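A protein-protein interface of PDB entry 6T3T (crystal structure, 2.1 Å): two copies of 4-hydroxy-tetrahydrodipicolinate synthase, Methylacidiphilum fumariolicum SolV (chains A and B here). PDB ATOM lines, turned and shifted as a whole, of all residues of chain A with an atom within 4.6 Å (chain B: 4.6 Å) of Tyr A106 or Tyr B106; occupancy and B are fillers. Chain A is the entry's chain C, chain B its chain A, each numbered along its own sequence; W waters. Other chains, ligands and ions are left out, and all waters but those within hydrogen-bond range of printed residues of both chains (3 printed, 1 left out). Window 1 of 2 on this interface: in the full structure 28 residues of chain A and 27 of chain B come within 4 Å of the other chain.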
ATOM      1  N   SER A  79     -15.350 -14.727   8.932  1.00  0.00           N
ATOM      2  CA  SER A  79     -16.266 -15.618   8.245  1.00  0.00           C
ATOM      3  C   SER A  79     -17.570 -15.587   9.020  1.00  0.00           C
ATOM      4  O   SER A  79     -17.595 -15.188  10.185  1.00  0.00           O
ATOM      5  CB  SER A  79     -15.698 -17.048   8.177  1.00  0.00           C
ATOM      6  OG  SER A  79     -16.677 -17.949   7.705  1.00  0.00           O
ATOM      7  N   ASN A  80     -18.650 -16.009   8.373  1.00  0.00           N
ATOM      8  CA  ASN A  80     -19.891 -16.226   9.113  1.00  0.00           C
ATOM      9  C   ASN A  80     -20.011 -17.643   9.654  1.00  0.00           C
ATOM     10  O   ASN A  80     -21.063 -17.996  10.190  1.00  0.00           O
ATOM     11  CB  ASN A  80     -21.112 -15.890   8.249  1.00  0.00           C
ATOM     12  CG  ASN A  80     -21.211 -16.768   7.011  1.00  0.00           C
ATOM     13  OD1 ASN A  80     -20.311 -17.565   6.724  1.00  0.00           O
ATOM     14  ND2 ASN A  80     -22.305 -16.620   6.268  1.00  0.00           N
ATOM     15  N   VAL A 103     -14.478  -9.405  10.195  1.00  0.00           N
ATOM     16  CA  VAL A 103     -15.811  -8.864   9.938  1.00  0.00           C
ATOM     17  C   VAL A 103     -16.823  -9.661  10.756  1.00  0.00           C
ATOM     18  O   VAL A 103     -16.645 -10.857  11.008  1.00  0.00           O
ATOM     19  CB  VAL A 103     -16.175  -8.885   8.442  1.00  0.00           C
ATOM     20  CG1 VAL A 103     -16.483 -10.302   7.967  1.00  0.00           C
ATOM     21  CG2 VAL A 103     -17.374  -7.987   8.162  1.00  0.00           C
ATOM     22  N   SER A 104     -17.887  -8.995  11.204  1.00  0.00           N
ATOM     23  CA  SER A 104     -18.910  -9.735  11.915  1.00  0.00           C
ATOM     24  C   SER A 104     -19.623 -10.682  10.949  1.00  0.00           C
ATOM     25  O   SER A 104     -19.718 -10.399   9.749  1.00  0.00           O
ATOM     26  CB  SER A 104     -19.909  -8.798  12.577  1.00  0.00           C
ATOM     27  OG  SER A 104     -20.657  -8.146  11.594  1.00  0.00           O
ATOM     28  N   PRO A 105     -20.095 -11.827  11.439  1.00  0.00           N
ATOM     29  CA  PRO A 105     -20.831 -12.755  10.576  1.00  0.00           C
ATOM     30  C   PRO A 105     -21.917 -12.059   9.769  1.00  0.00           C
ATOM     31  O   PRO A 105     -22.760 -11.334  10.315  1.00  0.00           O
ATOM     32  CB  PRO A 105     -21.422 -13.758  11.576  1.00  0.00           C
ATOM     33  CG  PRO A 105     -20.370 -13.800  12.651  1.00  0.00           C
ATOM     34  CD  PRO A 105     -19.913 -12.365  12.791  1.00  0.00           C
ATOM     35  N   TYR A 106     -21.905 -12.335   8.465  1.00  0.00           N
ATOM     36  CA  TYR A 106     -22.803 -11.776   7.462  1.00  0.00           C
ATOM     37  C   TYR A 106     -23.836 -12.830   7.098  1.00  0.00           C
ATOM     38  O   TYR A 106     -23.596 -14.038   7.244  1.00  0.00           O
ATOM     39  CB  TYR A 106     -21.979 -11.296   6.238  1.00  0.00           C
ATOM     40  CG  TYR A 106     -20.941 -12.321   5.808  1.00  0.00           C
ATOM     41  CD1 TYR A 106     -21.308 -13.542   5.241  1.00  0.00           C
ATOM     42  CD2 TYR A 106     -19.623 -12.159   6.169  1.00  0.00           C
ATOM     43  CE1 TYR A 106     -20.360 -14.507   4.911  1.00  0.00           C
ATOM     44  CE2 TYR A 106     -18.666 -13.137   5.882  1.00  0.00           C
ATOM     45  CZ  TYR A 106     -19.044 -14.311   5.245  1.00  0.00           C
ATOM     46  OH  TYR A 106     -18.121 -15.305   4.951  1.00  0.00           O
ATOM     47  N   TYR A 107     -25.015 -12.350   6.722  1.00  0.00           N
ATOM     48  CA  TYR A 107     -26.068 -13.205   6.161  1.00  0.00           C
ATOM     49  C   TYR A 107     -26.849 -14.004   7.211  1.00  0.00           C
ATOM     50  O   TYR A 107     -28.084 -13.970   7.182  1.00  0.00           O
ATOM     51  CB  TYR A 107     -25.472 -14.127   5.091  1.00  0.00           C
ATOM     52  CG  TYR A 107     -26.494 -14.975   4.396  1.00  0.00           C
ATOM     53  CD1 TYR A 107     -27.548 -14.384   3.698  1.00  0.00           C
ATOM     54  CD2 TYR A 107     -26.417 -16.351   4.426  1.00  0.00           C
ATOM     55  CE1 TYR A 107     -28.497 -15.147   3.058  1.00  0.00           C
ATOM     56  CE2 TYR A 107     -27.362 -17.129   3.782  1.00  0.00           C
ATOM     57  CZ  TYR A 107     -28.403 -16.516   3.106  1.00  0.00           C
ATOM     58  OH  TYR A 107     -29.360 -17.274   2.467  1.00  0.00           O
ATOM     59  N   ASN A 108     -26.197 -14.700   8.159  1.00  0.00           N
ATOM     60  CA  ASN A 108     -26.987 -15.481   9.119  1.00  0.00           C
ATOM     61  C   ASN A 108     -27.442 -14.676  10.343  1.00  0.00           C
ATOM     62  O   ASN A 108     -28.200 -15.201  11.168  1.00  0.00           O
ATOM     63  CB  ASN A 108     -26.250 -16.778   9.528  1.00  0.00           C
ATOM     64  CG  ASN A 108     -24.799 -16.555   9.967  1.00  0.00           C
ATOM     65  OD1 ASN A 108     -24.320 -15.435  10.028  1.00  0.00           O
ATOM     66  ND2 ASN A 108     -24.097 -17.650  10.259  1.00  0.00           N
ATOM     67  N   ARG A 138     -23.414  -4.406   4.795  1.00  0.00           N
ATOM     68  CA  ARG A 138     -23.050  -5.623   4.078  1.00  0.00           C
ATOM     69  C   ARG A 138     -23.438  -6.897   4.820  1.00  0.00           C
ATOM     70  O   ARG A 138     -23.642  -7.934   4.182  1.00  0.00           O
ATOM     71  CB  ARG A 138     -21.530  -5.656   3.824  1.00  0.00           C
ATOM     72  CG  ARG A 138     -20.996  -4.545   2.903  1.00  0.00           C
ATOM     73  CD  ARG A 138     -19.483  -4.711   2.695  1.00  0.00           C
ATOM     74  NE  ARG A 138     -18.928  -3.743   1.750  1.00  0.00           N
ATOM     75  CZ  ARG A 138     -18.840  -3.945   0.438  1.00  0.00           C
ATOM     76  NH1 ARG A 138     -19.263  -5.086  -0.094  1.00  0.00           N
ATOM     77  NH2 ARG A 138     -18.316  -3.016  -0.341  1.00  0.00           N
ATOM     78  N   CYS A 139     -23.531  -6.858   6.150  1.00  0.00           N
ATOM     79  CA  CYS A 139     -23.672  -8.084   6.926  1.00  0.00           C
ATOM     80  C   CYS A 139     -25.099  -8.401   7.321  1.00  0.00           C
ATOM     81  O   CYS A 139     -25.435  -9.582   7.458  1.00  0.00           O
ATOM     82  CB  CYS A 139     -22.829  -7.998   8.196  1.00  0.00           C
ATOM     83  SG  CYS A 139     -21.070  -7.986   7.883  1.00  0.00           S
ATOM     84  N   SER B  79     -24.507 -18.893  -3.527  1.00  0.00           N
ATOM     85  CA  SER B  79     -23.251 -18.480  -2.919  1.00  0.00           C
ATOM     86  C   SER B  79     -23.033 -17.036  -3.303  1.00  0.00           C
ATOM     87  O   SER B  79     -23.648 -16.535  -4.246  1.00  0.00           O
ATOM     88  CB  SER B  79     -22.060 -19.338  -3.387  1.00  0.00           C
ATOM     89  OG  SER B  79     -20.822 -18.752  -3.012  1.00  0.00           O
ATOM     90  N   ASN B  80     -22.180 -16.355  -2.560  1.00  0.00           N
ATOM     91  CA  ASN B  80     -21.797 -15.044  -3.038  1.00  0.00           C
ATOM     92  C   ASN B  80     -20.591 -15.103  -3.972  1.00  0.00           C
ATOM     93  O   ASN B  80     -20.140 -14.051  -4.426  1.00  0.00           O
ATOM     94  CB  ASN B  80     -21.564 -14.082  -1.882  1.00  0.00           C
ATOM     95  CG  ASN B  80     -20.447 -14.516  -0.965  1.00  0.00           C
ATOM     96  OD1 ASN B  80     -19.887 -15.603  -1.111  1.00  0.00           O
ATOM     97  ND2 ASN B  80     -20.099 -13.648  -0.016  1.00  0.00           N
ATOM     98  N   VAL B 103     -30.071 -17.959  -3.479  1.00  0.00           N
ATOM     99  CA  VAL B 103     -30.080 -16.704  -2.755  1.00  0.00           C
ATOM    100  C   VAL B 103     -29.203 -15.720  -3.496  1.00  0.00           C
ATOM    101  O   VAL B 103     -28.225 -16.094  -4.158  1.00  0.00           O
ATOM    102  CB  VAL B 103     -29.609 -16.898  -1.297  1.00  0.00           C
ATOM    103  CG1 VAL B 103     -28.137 -17.235  -1.223  1.00  0.00           C
ATOM    104  CG2 VAL B 103     -29.928 -15.653  -0.453  1.00  0.00           C
ATOM    105  N   SER B 104     -29.571 -14.445  -3.423  1.00  0.00           N
ATOM    106  CA  SER B 104     -28.723 -13.447  -4.036  1.00  0.00           C
ATOM    107  C   SER B 104     -27.396 -13.384  -3.283  1.00  0.00           C
ATOM    108  O   SER B 104     -27.335 -13.724  -2.096  1.00  0.00           O
ATOM    109  CB  SER B 104     -29.426 -12.081  -4.061  1.00  0.00           C
ATOM    110  OG  SER B 104     -29.513 -11.566  -2.766  1.00  0.00           O
ATOM    111  N   PRO B 105     -26.300 -13.055  -3.974  1.00  0.00           N
ATOM    112  CA  PRO B 105     -25.010 -12.904  -3.287  1.00  0.00           C
ATOM    113  C   PRO B 105     -25.148 -11.993  -2.077  1.00  0.00           C
ATOM    114  O   PRO B 105     -25.700 -10.895  -2.166  1.00  0.00           O
ATOM    115  CB  PRO B 105     -24.096 -12.290  -4.362  1.00  0.00           C
ATOM    116  CG  PRO B 105     -24.707 -12.749  -5.688  1.00  0.00           C
ATOM    117  CD  PRO B 105     -26.206 -12.824  -5.428  1.00  0.00           C
ATOM    118  N   TYR B 106     -24.622 -12.445  -0.948  1.00  0.00           N
ATOM    119  CA  TYR B 106     -24.670 -11.713   0.309  1.00  0.00           C
ATOM    120  C   TYR B 106     -23.310 -11.063   0.527  1.00  0.00           C
ATOM    121  O   TYR B 106     -22.302 -11.498  -0.043  1.00  0.00           O
ATOM    122  CB  TYR B 106     -25.003 -12.664   1.466  1.00  0.00           C
ATOM    123  CG  TYR B 106     -24.310 -13.992   1.287  1.00  0.00           C
ATOM    124  CD1 TYR B 106     -22.983 -14.174   1.667  1.00  0.00           C
ATOM    125  CD2 TYR B 106     -24.953 -15.037   0.655  1.00  0.00           C
ATOM    126  CE1 TYR B 106     -22.342 -15.377   1.477  1.00  0.00           C
ATOM    127  CE2 TYR B 106     -24.313 -16.234   0.444  1.00  0.00           C
ATOM    128  CZ  TYR B 106     -23.010 -16.396   0.848  1.00  0.00           C
ATOM    129  OH  TYR B 106     -22.377 -17.591   0.630  1.00  0.00           O
ATOM    130  N   TYR B 107     -23.314  -9.942   1.245  1.00  0.00           N
ATOM    131  CA  TYR B 107     -22.071  -9.319   1.701  1.00  0.00           C
ATOM    132  C   TYR B 107     -21.300  -8.531   0.640  1.00  0.00           C
ATOM    133  O   TYR B 107     -20.852  -7.426   0.939  1.00  0.00           O
ATOM    134  CB  TYR B 107     -21.130 -10.358   2.323  1.00  0.00           C
ATOM    135  CG  TYR B 107     -19.878  -9.724   2.915  1.00  0.00           C
ATOM    136  CD1 TYR B 107     -19.960  -8.824   3.983  1.00  0.00           C
ATOM    137  CD2 TYR B 107     -18.629 -10.003   2.396  1.00  0.00           C
ATOM    138  CE1 TYR B 107     -18.818  -8.238   4.530  1.00  0.00           C
ATOM    139  CE2 TYR B 107     -17.480  -9.423   2.929  1.00  0.00           C
ATOM    140  CZ  TYR B 107     -17.580  -8.539   3.993  1.00  0.00           C
ATOM    141  OH  TYR B 107     -16.433  -7.966   4.504  1.00  0.00           O
ATOM    142  N   ASN B 108     -21.085  -9.056  -0.573  1.00  0.00           N
ATOM    143  CA  ASN B 108     -20.303  -8.271  -1.533  1.00  0.00           C
ATOM    144  C   ASN B 108     -21.142  -7.286  -2.351  1.00  0.00           C
ATOM    145  O   ASN B 108     -20.570  -6.512  -3.132  1.00  0.00           O
ATOM    146  CB  ASN B 108     -19.444  -9.182  -2.466  1.00  0.00           C
ATOM    147  CG  ASN B 108     -20.227 -10.344  -3.141  1.00  0.00           C
ATOM    148  OD1 ASN B 108     -21.456 -10.453  -3.052  1.00  0.00           O
ATOM    149  ND2 ASN B 108     -19.476 -11.233  -3.809  1.00  0.00           N
ATOM    150  N   ARG B 138     -30.813  -9.954   4.886  1.00  0.00           N
ATOM    151  CA  ARG B 138     -29.656 -10.799   5.134  1.00  0.00           C
ATOM    152  C   ARG B 138     -28.541 -10.581   4.120  1.00  0.00           C
ATOM    153  O   ARG B 138     -27.382 -10.866   4.424  1.00  0.00           O
ATOM    154  CB  ARG B 138     -30.053 -12.284   5.144  1.00  0.00           C
ATOM    155  CG  ARG B 138     -30.974 -12.732   6.283  1.00  0.00           C
ATOM    156  CD  ARG B 138     -31.353 -14.169   6.058  1.00  0.00           C
ATOM    157  NE  ARG B 138     -32.226 -14.728   7.090  1.00  0.00           N
ATOM    158  CZ  ARG B 138     -31.793 -15.257   8.235  1.00  0.00           C
ATOM    159  NH1 ARG B 138     -30.482 -15.290   8.516  1.00  0.00           N
ATOM    160  NH2 ARG B 138     -32.678 -15.757   9.097  1.00  0.00           N
ATOM    161  N   CYS B 139     -28.859 -10.131   2.913  1.00  0.00           N
ATOM    162  CA  CYS B 139     -27.868 -10.064   1.850  1.00  0.00           C
ATOM    163  C   CYS B 139     -27.254  -8.686   1.705  1.00  0.00           C
ATOM    164  O   CYS B 139     -26.095  -8.579   1.307  1.00  0.00           O
ATOM    165  CB  CYS B 139     -28.497 -10.493   0.518  1.00  0.00           C
ATOM    166  SG  CYS B 139     -28.973 -12.253   0.495  1.00  0.00           S
HETATM  167  O   HOH W   1     -17.893  -6.061  -2.755  1.00  0.00           O
HETATM  168  O   HOH W   2     -29.280 -17.659  10.512  1.00  0.00           O
HETATM  169  O   HOH W   3     -17.901 -13.927   1.960  1.00  0.00           O
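Printed residues of chain B within 4 Å of Tyr A106: Tyr B106 (3.997 Å) and Tyr B107 (3.9 Å).
Printed residues of chain A within 4 Å of Tyr B106: Tyr A106 and Tyr A107.
Of the printed residues of chain B, Cys A139 touches Arg B138.
Of the printed residues of chain B, Tyr A107 touches Val B103, Tyr B106, Arg B138 and Cys B139.
Printed residues of chain B within 4 Å of Asn A108: Arg B138 (3.5 Å).
Printed residues of chain A within 4 Å of Tyr B107: Val A103 (3.8 Å), Tyr A106 (3.9 Å) and Arg A138 (3.0 Å).
Ser B104 touches none of the printed residues of chain A.
The nearest printed residue of chain B that does not touch Val A103 is Asn B80 (9.4 Å).
Among the printed residues, pairs that only touch across the chains: Tyr A107 with Val B103, Arg A138 with Asn B108, Val A103 with Tyr B107, Tyr A107 with Tyr B106, Cys A139 with Arg B138, Arg A138 with Cys B139, Tyr A107 with Cys B139, Tyr A106 with Tyr B107 and Tyr A106 with Tyr B106.
Of the 10 printed residues of chain A, 6 touch a printed residue of chain B.
Hydrophobic or aromatic side chains of chain A that line the printed part of chain B: Val A103, Tyr A106 and Tyr A107.
Hydrophobic or aromatic side chains of chain B that line the printed part of chain A: Val B103, Tyr B106 and Tyr B107.
Among the printed residues, no Asp or Glu carboxylate lies within 4 Å of a Lys or Arg side-chain nitrogen of the other chain.
N of Tyr A107 is in hydrogen-bond range of O of Cys A139, 2.9 Å away.
The side-chain hydroxyl of Ser B104 sits at hydrogen-bond distance from the side-chain sulfur of Cys B139.
The side-chain amide nitrogen (ND2) of Asn B108 sits at hydrogen-bond distance from the backbone carbonyl oxygen (O) of Asn B80, at 3.0 Å.
The side-chain sulfur of Cys A139 lies within hydrogen-bond range of the backbone carbonyl oxygen of Ser A104 (3.3 Å).
The backbone carbonyl oxygen of Tyr A106 lies close to the side-chain amide oxygen of Asn A108, 3.2 Å away.
The side-chain amide nitrogen of Asn B80 is in hydrogen-bond range of the backbone carbonyl oxygen of Tyr B106 (3.1 Å).
Water W1 bridges the backbone carbonyl oxygen of Asn B108 (2.7 Å) and the guanidinium group of Arg A138 (3.1 Å).
Water W2 bridges O of Asn A108 (2.8 Å) and NH1 of Arg B138 (3.3 Å).
Water W3 bridges the side-chain amide nitrogen (ND2) of Asn B80 (3.0 Å) and the side-chain hydroxyl (OH) of Tyr A106 (3.3 Å).
The backbone carbonyl oxygen (O) of Asn A108 lies within hydrogen-bond range of the guanidinium group (NH1) of Arg B138 (3.5 Å).
The backbone carbonyl oxygen of Tyr B107 lies within hydrogen-bond range of the guanidinium group of Arg A138, at 3.0 Å.
O of Tyr A107 is in hydrogen-bond range of NH1 of Arg B138 (3.0 Å).
Tyr A106 touches its own counterpart, Tyr B106.
Tyr A107 touches Cys B139, but with the chains exchanged Cys A139 does not touch Tyr B107 (4.05 Å).
Asn A108 touches Arg B138, and with the chains exchanged Arg A138 touches Asn B108.
Arg A138 touches Cys B139, and with the chains exchanged Cys A139 touches Arg B138.
Of the 12 pairs that touch across the chains among the printed residues, 11 have their exchanged pair printed and touching as well.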
